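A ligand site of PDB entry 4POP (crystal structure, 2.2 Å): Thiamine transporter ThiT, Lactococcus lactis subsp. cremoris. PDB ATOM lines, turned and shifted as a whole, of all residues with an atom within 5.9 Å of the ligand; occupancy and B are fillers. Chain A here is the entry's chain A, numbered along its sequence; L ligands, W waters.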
ATOM      1  N   TRP A  44       1.868   6.826  29.216  1.00  0.00           N
ATOM      2  CA  TRP A  44       1.969   7.966  28.305  1.00  0.00           C
ATOM      3  C   TRP A  44       2.911   9.036  28.870  1.00  0.00           C
ATOM      4  O   TRP A  44       2.936  10.160  28.379  1.00  0.00           O
ATOM      5  CB  TRP A  44       0.579   8.523  27.992  1.00  0.00           C
ATOM      6  CG  TRP A  44       0.013   8.042  26.654  1.00  0.00           C
ATOM      7  CD1 TRP A  44      -1.009   7.181  26.457  1.00  0.00           C
ATOM      8  CD2 TRP A  44       0.474   8.427  25.346  1.00  0.00           C
ATOM      9  NE1 TRP A  44      -1.224   6.990  25.119  1.00  0.00           N
ATOM     10  CE2 TRP A  44      -0.336   7.746  24.406  1.00  0.00           C
ATOM     11  CE3 TRP A  44       1.468   9.277  24.878  1.00  0.00           C
ATOM     12  CZ2 TRP A  44      -0.182   7.885  23.017  1.00  0.00           C
ATOM     13  CZ3 TRP A  44       1.637   9.424  23.492  1.00  0.00           C
ATOM     14  CH2 TRP A  44       0.824   8.722  22.582  1.00  0.00           C
ATOM     15  N   ILE A  46       6.406  10.246  28.681  1.00  0.00           N
ATOM     16  CA  ILE A  46       7.350  10.072  27.607  1.00  0.00           C
ATOM     17  C   ILE A  46       8.381  11.183  27.576  1.00  0.00           C
ATOM     18  O   ILE A  46       8.176  12.296  28.138  1.00  0.00           O
ATOM     19  CB  ILE A  46       6.630  10.015  26.237  1.00  0.00           C
ATOM     20  CG1 ILE A  46       5.883  11.332  25.936  1.00  0.00           C
ATOM     21  CG2 ILE A  46       5.660   8.823  26.169  1.00  0.00           C
ATOM     22  CD1 ILE A  46       5.402  11.425  24.448  1.00  0.00           C
ATOM     23  N   GLU A  48       9.868  13.329  24.777  1.00  0.00           N
ATOM     24  CA  GLU A  48       9.679  13.582  23.339  1.00  0.00           C
ATOM     25  C   GLU A  48      10.886  14.283  22.662  1.00  0.00           C
ATOM     26  O   GLU A  48      10.820  15.441  22.273  1.00  0.00           O
ATOM     27  CB  GLU A  48       8.396  14.405  23.092  1.00  0.00           C
ATOM     28  CG  GLU A  48       8.023  14.416  21.590  1.00  0.00           C
ATOM     29  CD  GLU A  48       6.596  14.820  21.316  1.00  0.00           C
ATOM     30  OE1 GLU A  48       6.107  15.737  22.014  1.00  0.00           O
ATOM     31  OE2 GLU A  48       5.974  14.224  20.415  1.00  0.00           O
ATOM     32  N   TYR A  84      -1.356   8.325  17.483  1.00  0.00           N
ATOM     33  CA  TYR A  84      -2.452   7.710  18.252  1.00  0.00           C
ATOM     34  C   TYR A  84      -3.702   8.612  18.221  1.00  0.00           C
ATOM     35  O   TYR A  84      -3.754   9.667  18.857  1.00  0.00           O
ATOM     36  CB  TYR A  84      -2.002   7.436  19.689  1.00  0.00           C
ATOM     37  CG  TYR A  84      -0.841   6.470  19.777  1.00  0.00           C
ATOM     38  CD1 TYR A  84       0.476   6.909  19.627  1.00  0.00           C
ATOM     39  CD2 TYR A  84      -1.055   5.102  19.978  1.00  0.00           C
ATOM     40  CE1 TYR A  84       1.529   6.010  19.691  1.00  0.00           C
ATOM     41  CE2 TYR A  84       0.003   4.215  20.047  1.00  0.00           C
ATOM     42  CZ  TYR A  84       1.288   4.679  19.908  1.00  0.00           C
ATOM     43  OH  TYR A  84       2.341   3.807  19.985  1.00  0.00           O
ATOM     44  N   GLN A  90      -9.416  15.420  18.372  1.00  0.00           N
ATOM     45  CA  GLN A  90      -8.261  15.080  19.204  1.00  0.00           C
ATOM     46  C   GLN A  90      -6.982  14.998  18.396  1.00  0.00           C
ATOM     47  O   GLN A  90      -5.927  15.405  18.877  1.00  0.00           O
ATOM     48  CB  GLN A  90      -8.485  13.777  19.985  1.00  0.00           C
ATOM     49  CG  GLN A  90      -7.213  13.290  20.734  1.00  0.00           C
ATOM     50  CD  GLN A  90      -6.322  12.406  19.857  1.00  0.00           C
ATOM     51  OE1 GLN A  90      -6.783  11.812  18.887  1.00  0.00           O
ATOM     52  NE2 GLN A  90      -5.036  12.333  20.181  1.00  0.00           N
ATOM     53  N   GLU A  94      -3.802  17.290  18.887  1.00  0.00           N
ATOM     54  CA  GLU A  94      -2.545  16.701  19.380  1.00  0.00           C
ATOM     55  C   GLU A  94      -1.510  16.455  18.304  1.00  0.00           C
ATOM     56  O   GLU A  94      -0.315  16.282  18.621  1.00  0.00           O
ATOM     57  CB  GLU A  94      -2.813  15.390  20.111  1.00  0.00           C
ATOM     58  CG  GLU A  94      -3.620  15.577  21.393  1.00  0.00           C
ATOM     59  CD  GLU A  94      -3.403  14.439  22.398  1.00  0.00           C
ATOM     60  OE1 GLU A  94      -2.352  14.421  23.065  1.00  0.00           O
ATOM     61  OE2 GLU A  94      -4.269  13.560  22.534  1.00  0.00           O
ATOM     62  N   TYR A  95      -1.925  16.446  17.049  1.00  0.00           N
ATOM     63  CA  TYR A  95      -0.970  16.245  15.970  1.00  0.00           C
ATOM     64  C   TYR A  95      -0.957  17.374  14.946  1.00  0.00           C
ATOM     65  O   TYR A  95      -0.219  17.287  13.935  1.00  0.00           O
ATOM     66  CB  TYR A  95      -1.257  14.900  15.288  1.00  0.00           C
ATOM     67  CG  TYR A  95      -0.858  13.757  16.166  1.00  0.00           C
ATOM     68  CD1 TYR A  95       0.474  13.384  16.314  1.00  0.00           C
ATOM     69  CD2 TYR A  95      -1.817  13.043  16.874  1.00  0.00           C
ATOM     70  CE1 TYR A  95       0.834  12.315  17.124  1.00  0.00           C
ATOM     71  CE2 TYR A  95      -1.470  11.998  17.680  1.00  0.00           C
ATOM     72  CZ  TYR A  95      -0.162  11.631  17.800  1.00  0.00           C
ATOM     73  OH  TYR A  95       0.108  10.547  18.619  1.00  0.00           O
ATOM     74  N   LYS A 131       3.433  23.164  24.038  1.00  0.00           N
ATOM     75  CA  LYS A 131       3.071  21.875  23.490  1.00  0.00           C
ATOM     76  C   LYS A 131       2.351  21.030  24.566  1.00  0.00           C
ATOM     77  O   LYS A 131       1.286  20.499  24.294  1.00  0.00           O
ATOM     78  CB  LYS A 131       4.286  21.144  22.939  1.00  0.00           C
ATOM     79  CG  LYS A 131       3.888  20.014  22.020  1.00  0.00           C
ATOM     80  CD  LYS A 131       5.058  19.316  21.383  1.00  0.00           C
ATOM     81  CE  LYS A 131       4.604  18.483  20.196  1.00  0.00           C
ATOM     82  NZ  LYS A 131       4.222  17.067  20.460  1.00  0.00           N
ATOM     83  N   TYR A 132       2.880  20.950  25.796  1.00  0.00           N
ATOM     84  CA  TYR A 132       2.359  19.918  26.725  1.00  0.00           C
ATOM     85  C   TYR A 132       1.143  20.477  27.454  1.00  0.00           C
ATOM     86  O   TYR A 132       0.307  19.747  27.969  1.00  0.00           O
ATOM     87  CB  TYR A 132       3.490  19.390  27.626  1.00  0.00           C
ATOM     88  CG  TYR A 132       4.127  18.269  26.835  1.00  0.00           C
ATOM     89  CD1 TYR A 132       5.129  18.499  25.883  1.00  0.00           C
ATOM     90  CD2 TYR A 132       3.628  16.957  26.945  1.00  0.00           C
ATOM     91  CE1 TYR A 132       5.658  17.414  25.078  1.00  0.00           C
ATOM     92  CE2 TYR A 132       4.129  15.927  26.173  1.00  0.00           C
ATOM     93  CZ  TYR A 132       5.131  16.146  25.246  1.00  0.00           C
ATOM     94  OH  TYR A 132       5.572  15.050  24.514  1.00  0.00           O
ATOM     95  N   PHE A 134      -1.275  21.847  25.515  1.00  0.00           N
ATOM     96  CA  PHE A 134      -2.325  21.308  24.641  1.00  0.00           C
ATOM     97  C   PHE A 134      -2.558  19.792  24.851  1.00  0.00           C
ATOM     98  O   PHE A 134      -3.704  19.343  24.826  1.00  0.00           O
ATOM     99  CB  PHE A 134      -1.993  21.560  23.162  1.00  0.00           C
ATOM    100  CG  PHE A 134      -2.136  23.023  22.749  1.00  0.00           C
ATOM    101  CD1 PHE A 134      -3.349  23.688  22.874  1.00  0.00           C
ATOM    102  CD2 PHE A 134      -1.051  23.721  22.250  1.00  0.00           C
ATOM    103  CE1 PHE A 134      -3.448  25.011  22.505  1.00  0.00           C
ATOM    104  CE2 PHE A 134      -1.167  25.026  21.882  1.00  0.00           C
ATOM    105  CZ  PHE A 134      -2.352  25.676  22.015  1.00  0.00           C
ATOM    106  N   HIS A 135      -1.488  19.006  25.037  1.00  0.00           N
ATOM    107  CA  HIS A 135      -1.638  17.589  25.410  1.00  0.00           C
ATOM    108  C   HIS A 135      -2.393  17.428  26.727  1.00  0.00           C
ATOM    109  O   HIS A 135      -3.226  16.545  26.877  1.00  0.00           O
ATOM    110  CB  HIS A 135      -0.290  16.898  25.506  1.00  0.00           C
ATOM    111  CG  HIS A 135       0.426  16.796  24.200  1.00  0.00           C
ATOM    112  ND1 HIS A 135      -0.130  16.245  23.079  1.00  0.00           N
ATOM    113  CD2 HIS A 135       1.664  17.234  23.832  1.00  0.00           C
ATOM    114  CE1 HIS A 135       0.738  16.304  22.080  1.00  0.00           C
ATOM    115  NE2 HIS A 135       1.832  16.896  22.520  1.00  0.00           N
ATOM    116  N   PHE A 136      -2.108  18.321  27.670  1.00  0.00           N
ATOM    117  CA  PHE A 136      -2.812  18.326  28.939  1.00  0.00           C
ATOM    118  C   PHE A 136      -4.292  18.622  28.772  1.00  0.00           C
ATOM    119  O   PHE A 136      -5.125  18.030  29.458  1.00  0.00           O
ATOM    120  CB  PHE A 136      -2.163  19.348  29.910  1.00  0.00           C
ATOM    121  CG  PHE A 136      -3.070  19.811  31.030  1.00  0.00           C
ATOM    122  CD1 PHE A 136      -3.411  18.950  32.091  1.00  0.00           C
ATOM    123  CD2 PHE A 136      -3.565  21.117  31.042  1.00  0.00           C
ATOM    124  CE1 PHE A 136      -4.218  19.396  33.134  1.00  0.00           C
ATOM    125  CE2 PHE A 136      -4.372  21.569  32.072  1.00  0.00           C
ATOM    126  CZ  PHE A 136      -4.710  20.717  33.129  1.00  0.00           C
ATOM    127  N   ALA A 138      -5.899  17.953  25.981  1.00  0.00           N
ATOM    128  CA  ALA A 138      -6.316  16.706  25.336  1.00  0.00           C
ATOM    129  C   ALA A 138      -6.576  15.607  26.366  1.00  0.00           C
ATOM    130  O   ALA A 138      -7.508  14.801  26.201  1.00  0.00           O
ATOM    131  CB  ALA A 138      -5.285  16.217  24.374  1.00  0.00           C
ATOM    132  N   GLY A 139      -5.717  15.554  27.383  1.00  0.00           N
ATOM    133  CA  GLY A 139      -5.709  14.457  28.336  1.00  0.00           C
ATOM    134  C   GLY A 139      -7.013  14.472  29.074  1.00  0.00           C
ATOM    135  O   GLY A 139      -7.654  13.441  29.273  1.00  0.00           O
ATOM    136  N   ILE A 140      -7.444  15.678  29.429  1.00  0.00           N
ATOM    137  CA  ILE A 140      -8.696  15.896  30.096  1.00  0.00           C
ATOM    138  C   ILE A 140      -9.898  15.522  29.242  1.00  0.00           C
ATOM    139  O   ILE A 140     -10.840  14.924  29.732  1.00  0.00           O
ATOM    140  CB  ILE A 140      -8.867  17.377  30.514  1.00  0.00           C
ATOM    141  CG1 ILE A 140      -7.773  17.775  31.511  1.00  0.00           C
ATOM    142  CG2 ILE A 140     -10.270  17.543  31.165  1.00  0.00           C
ATOM    143  CD1 ILE A 140      -7.763  19.234  31.896  1.00  0.00           C
ATOM    144  N   TRP A 143      -8.591  11.475  27.181  1.00  0.00           N
ATOM    145  CA  TRP A 143      -7.857  10.356  27.759  1.00  0.00           C
ATOM    146  C   TRP A 143      -8.268   9.995  29.187  1.00  0.00           C
ATOM    147  O   TRP A 143      -7.615   9.166  29.811  1.00  0.00           O
ATOM    148  CB  TRP A 143      -6.338  10.641  27.733  1.00  0.00           C
ATOM    149  CG  TRP A 143      -5.806  10.794  26.318  1.00  0.00           C
ATOM    150  CD1 TRP A 143      -5.670  11.966  25.616  1.00  0.00           C
ATOM    151  CD2 TRP A 143      -5.402   9.730  25.421  1.00  0.00           C
ATOM    152  NE1 TRP A 143      -5.205  11.691  24.341  1.00  0.00           N
ATOM    153  CE2 TRP A 143      -5.040  10.338  24.198  1.00  0.00           C
ATOM    154  CE3 TRP A 143      -5.290   8.346  25.544  1.00  0.00           C
ATOM    155  CZ2 TRP A 143      -4.545   9.609  23.120  1.00  0.00           C
ATOM    156  CZ3 TRP A 143      -4.834   7.615  24.434  1.00  0.00           C
ATOM    157  CH2 TRP A 143      -4.453   8.256  23.250  1.00  0.00           C
ATOM    158  N   TYR A 156      -4.916  13.566  36.912  1.00  0.00           N
ATOM    159  CA  TYR A 156      -4.287  12.618  36.021  1.00  0.00           C
ATOM    160  C   TYR A 156      -3.535  13.268  34.848  1.00  0.00           C
ATOM    161  O   TYR A 156      -2.396  12.905  34.589  1.00  0.00           O
ATOM    162  CB  TYR A 156      -5.326  11.699  35.456  1.00  0.00           C
ATOM    163  CG  TYR A 156      -4.782  10.693  34.500  1.00  0.00           C
ATOM    164  CD1 TYR A 156      -3.751   9.830  34.875  1.00  0.00           C
ATOM    165  CD2 TYR A 156      -5.328  10.562  33.236  1.00  0.00           C
ATOM    166  CE1 TYR A 156      -3.264   8.872  33.996  1.00  0.00           C
ATOM    167  CE2 TYR A 156      -4.862   9.602  32.364  1.00  0.00           C
ATOM    168  CZ  TYR A 156      -3.835   8.760  32.733  1.00  0.00           C
ATOM    169  OH  TYR A 156      -3.390   7.821  31.816  1.00  0.00           O
ATOM    170  N   SER A 157      -4.223  14.126  34.082  1.00  0.00           N
ATOM    171  CA  SER A 157      -3.628  14.717  32.874  1.00  0.00           C
ATOM    172  C   SER A 157      -2.456  15.622  33.232  1.00  0.00           C
ATOM    173  O   SER A 157      -1.487  15.699  32.482  1.00  0.00           O
ATOM    174  CB  SER A 157      -4.665  15.512  32.087  1.00  0.00           C
ATOM    175  OG  SER A 157      -4.131  15.871  30.821  1.00  0.00           O
ATOM    176  N   VAL A 160       0.667  13.124  34.090  1.00  0.00           N
ATOM    177  CA  VAL A 160       1.162  12.517  32.873  1.00  0.00           C
ATOM    178  C   VAL A 160       1.809  13.578  31.996  1.00  0.00           C
ATOM    179  O   VAL A 160       2.962  13.415  31.579  1.00  0.00           O
ATOM    180  CB  VAL A 160       0.067  11.815  32.087  1.00  0.00           C
ATOM    181  CG1 VAL A 160       0.548  11.423  30.704  1.00  0.00           C
ATOM    182  CG2 VAL A 160      -0.450  10.525  32.883  1.00  0.00           C
ATOM    183  N   ASN A 161       1.077  14.646  31.675  1.00  0.00           N
ATOM    184  CA  ASN A 161       1.592  15.559  30.645  1.00  0.00           C
ATOM    185  C   ASN A 161       2.555  16.626  31.271  1.00  0.00           C
ATOM    186  O   ASN A 161       3.574  16.990  30.651  1.00  0.00           O
ATOM    187  CB  ASN A 161       0.438  16.177  29.863  1.00  0.00           C
ATOM    188  CG  ASN A 161      -0.332  15.158  29.057  1.00  0.00           C
ATOM    189  OD1 ASN A 161       0.212  14.557  28.130  1.00  0.00           O
ATOM    190  ND2 ASN A 161      -1.614  14.974  29.386  1.00  0.00           N
ATOM    191  N   SER A 164       5.736  14.486  31.304  1.00  0.00           N
ATOM    192  CA  SER A 164       6.296  14.422  29.954  1.00  0.00           C
ATOM    193  C   SER A 164       6.925  15.737  29.511  1.00  0.00           C
ATOM    194  O   SER A 164       8.015  15.751  28.911  1.00  0.00           O
ATOM    195  CB  SER A 164       5.221  14.017  28.954  1.00  0.00           C
ATOM    196  OG  SER A 164       4.869  12.663  29.200  1.00  0.00           O
HETATM  197  C1  LIG L   1      -3.331  11.407  29.797  1.00  0.00           C
HETATM  198  N1  LIG L   1      -2.582  14.037  25.835  1.00  0.00           N
HETATM  199  C2  LIG L   1      -0.512  12.147  21.593  1.00  0.00           C
HETATM  200  O1  LIG L   1       2.302  12.825  20.728  1.00  0.00           O
HETATM  201  C3  LIG L   1       2.483  13.526  21.917  1.00  0.00           C
HETATM  202  C4  LIG L   1       0.396  12.644  25.285  1.00  0.00           C
HETATM  203  S1  LIG L   1       1.824  13.277  24.601  1.00  0.00           S
HETATM  204  C5  LIG L   1       1.501  13.091  22.986  1.00  0.00           C
HETATM  205  C6  LIG L   1       0.217  12.492  22.908  1.00  0.00           C
HETATM  206  C7  LIG L   1      -0.398  12.235  24.174  1.00  0.00           C
HETATM  207  C8  LIG L   1      -1.794  11.605  24.269  1.00  0.00           C
HETATM  208  C9  LIG L   1      -2.556  12.765  26.437  1.00  0.00           C
HETATM  209  N2  LIG L   1      -2.911  12.653  27.723  1.00  0.00           N
HETATM  210  C10 LIG L   1      -2.926  11.467  28.340  1.00  0.00           C
HETATM  211  N3  LIG L   1      -2.599  10.361  27.720  1.00  0.00           N
HETATM  212  C11 LIG L   1      -2.251  10.338  26.427  1.00  0.00           C
HETATM  213  C12 LIG L   1      -2.205  11.585  25.736  1.00  0.00           C
HETATM  214  O   HOH W   1       2.471  13.006  27.936  1.00  0.00           O
HETATM  215  O   HOH W   2      -3.806   8.310  29.140  1.00  0.00           O
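The side-chain carboxylate of Glu 48 is in salt-bridge range of the side-chain amino group of Lys 131 (2.8 Å). The backbone carbonyl oxygen of His 135 is in hydrogen-bond range of the side-chain amide nitrogen of Asn 161, at 3.4 Å. The side-chain carboxylate of Glu 94 is in hydrogen-bond range of the indole nitrogen of Trp 143 (2.8 Å). The backbone carbonyl oxygen of Val 160 lies within hydrogen-bond range of the side-chain hydroxyl of Ser 164 (3.1 Å). OE1 of Glu 48 is in hydrogen-bond range of OH of Tyr 132 (2.6 Å). The side-chain carboxylate of Glu 94 lies within hydrogen-bond range of a ring nitrogen (ND1) of His 135 (2.9 Å). A ring nitrogen (NE2) of His 135 sits at hydrogen-bond distance from the side-chain amino group of Lys 131 (3.2 Å). The side-chain hydroxyl (OG) of Ser 164 sits at hydrogen-bond distance from the backbone carbonyl oxygen (O) of Trp 44 (3.3 Å).
Merely in contact with the ligand: Trp 44, Glu 48, Tyr 95, Tyr 132, Ala 138, Gly 139, Trp 143, Tyr 156 and Val 160. Hydrophobic or aromatic side chains that line the ligand: Trp 44, Tyr 95, Tyr 132, His 135, Ala 138, Trp 143, Tyr 156 and Val 160. 12 residues have an atom within 4 Å of the ligand: Trp 44, Glu 48, Glu 94, Tyr 95, Tyr 132, His 135, Ala 138, Gly 139, Trp 143, Tyr 156, Val 160 and Asn 161.
N1 of the ligand lies within hydrogen-bond range of O of His 135 (2.8 Å). The side-chain carboxylate (OE1) of Glu 94 lies within hydrogen-bond range of a nitrogen (N1) of the ligand, at 2.8 Å. ND2 of Asn 161 lies within hydrogen-bond range of N2 of the ligand (3.1 Å).
Water W2 lies within hydrogen-bond range of the side-chain hydroxyl of Tyr 156 (2.8 Å) and a nitrogen (N3) of the ligand (2.8 Å).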
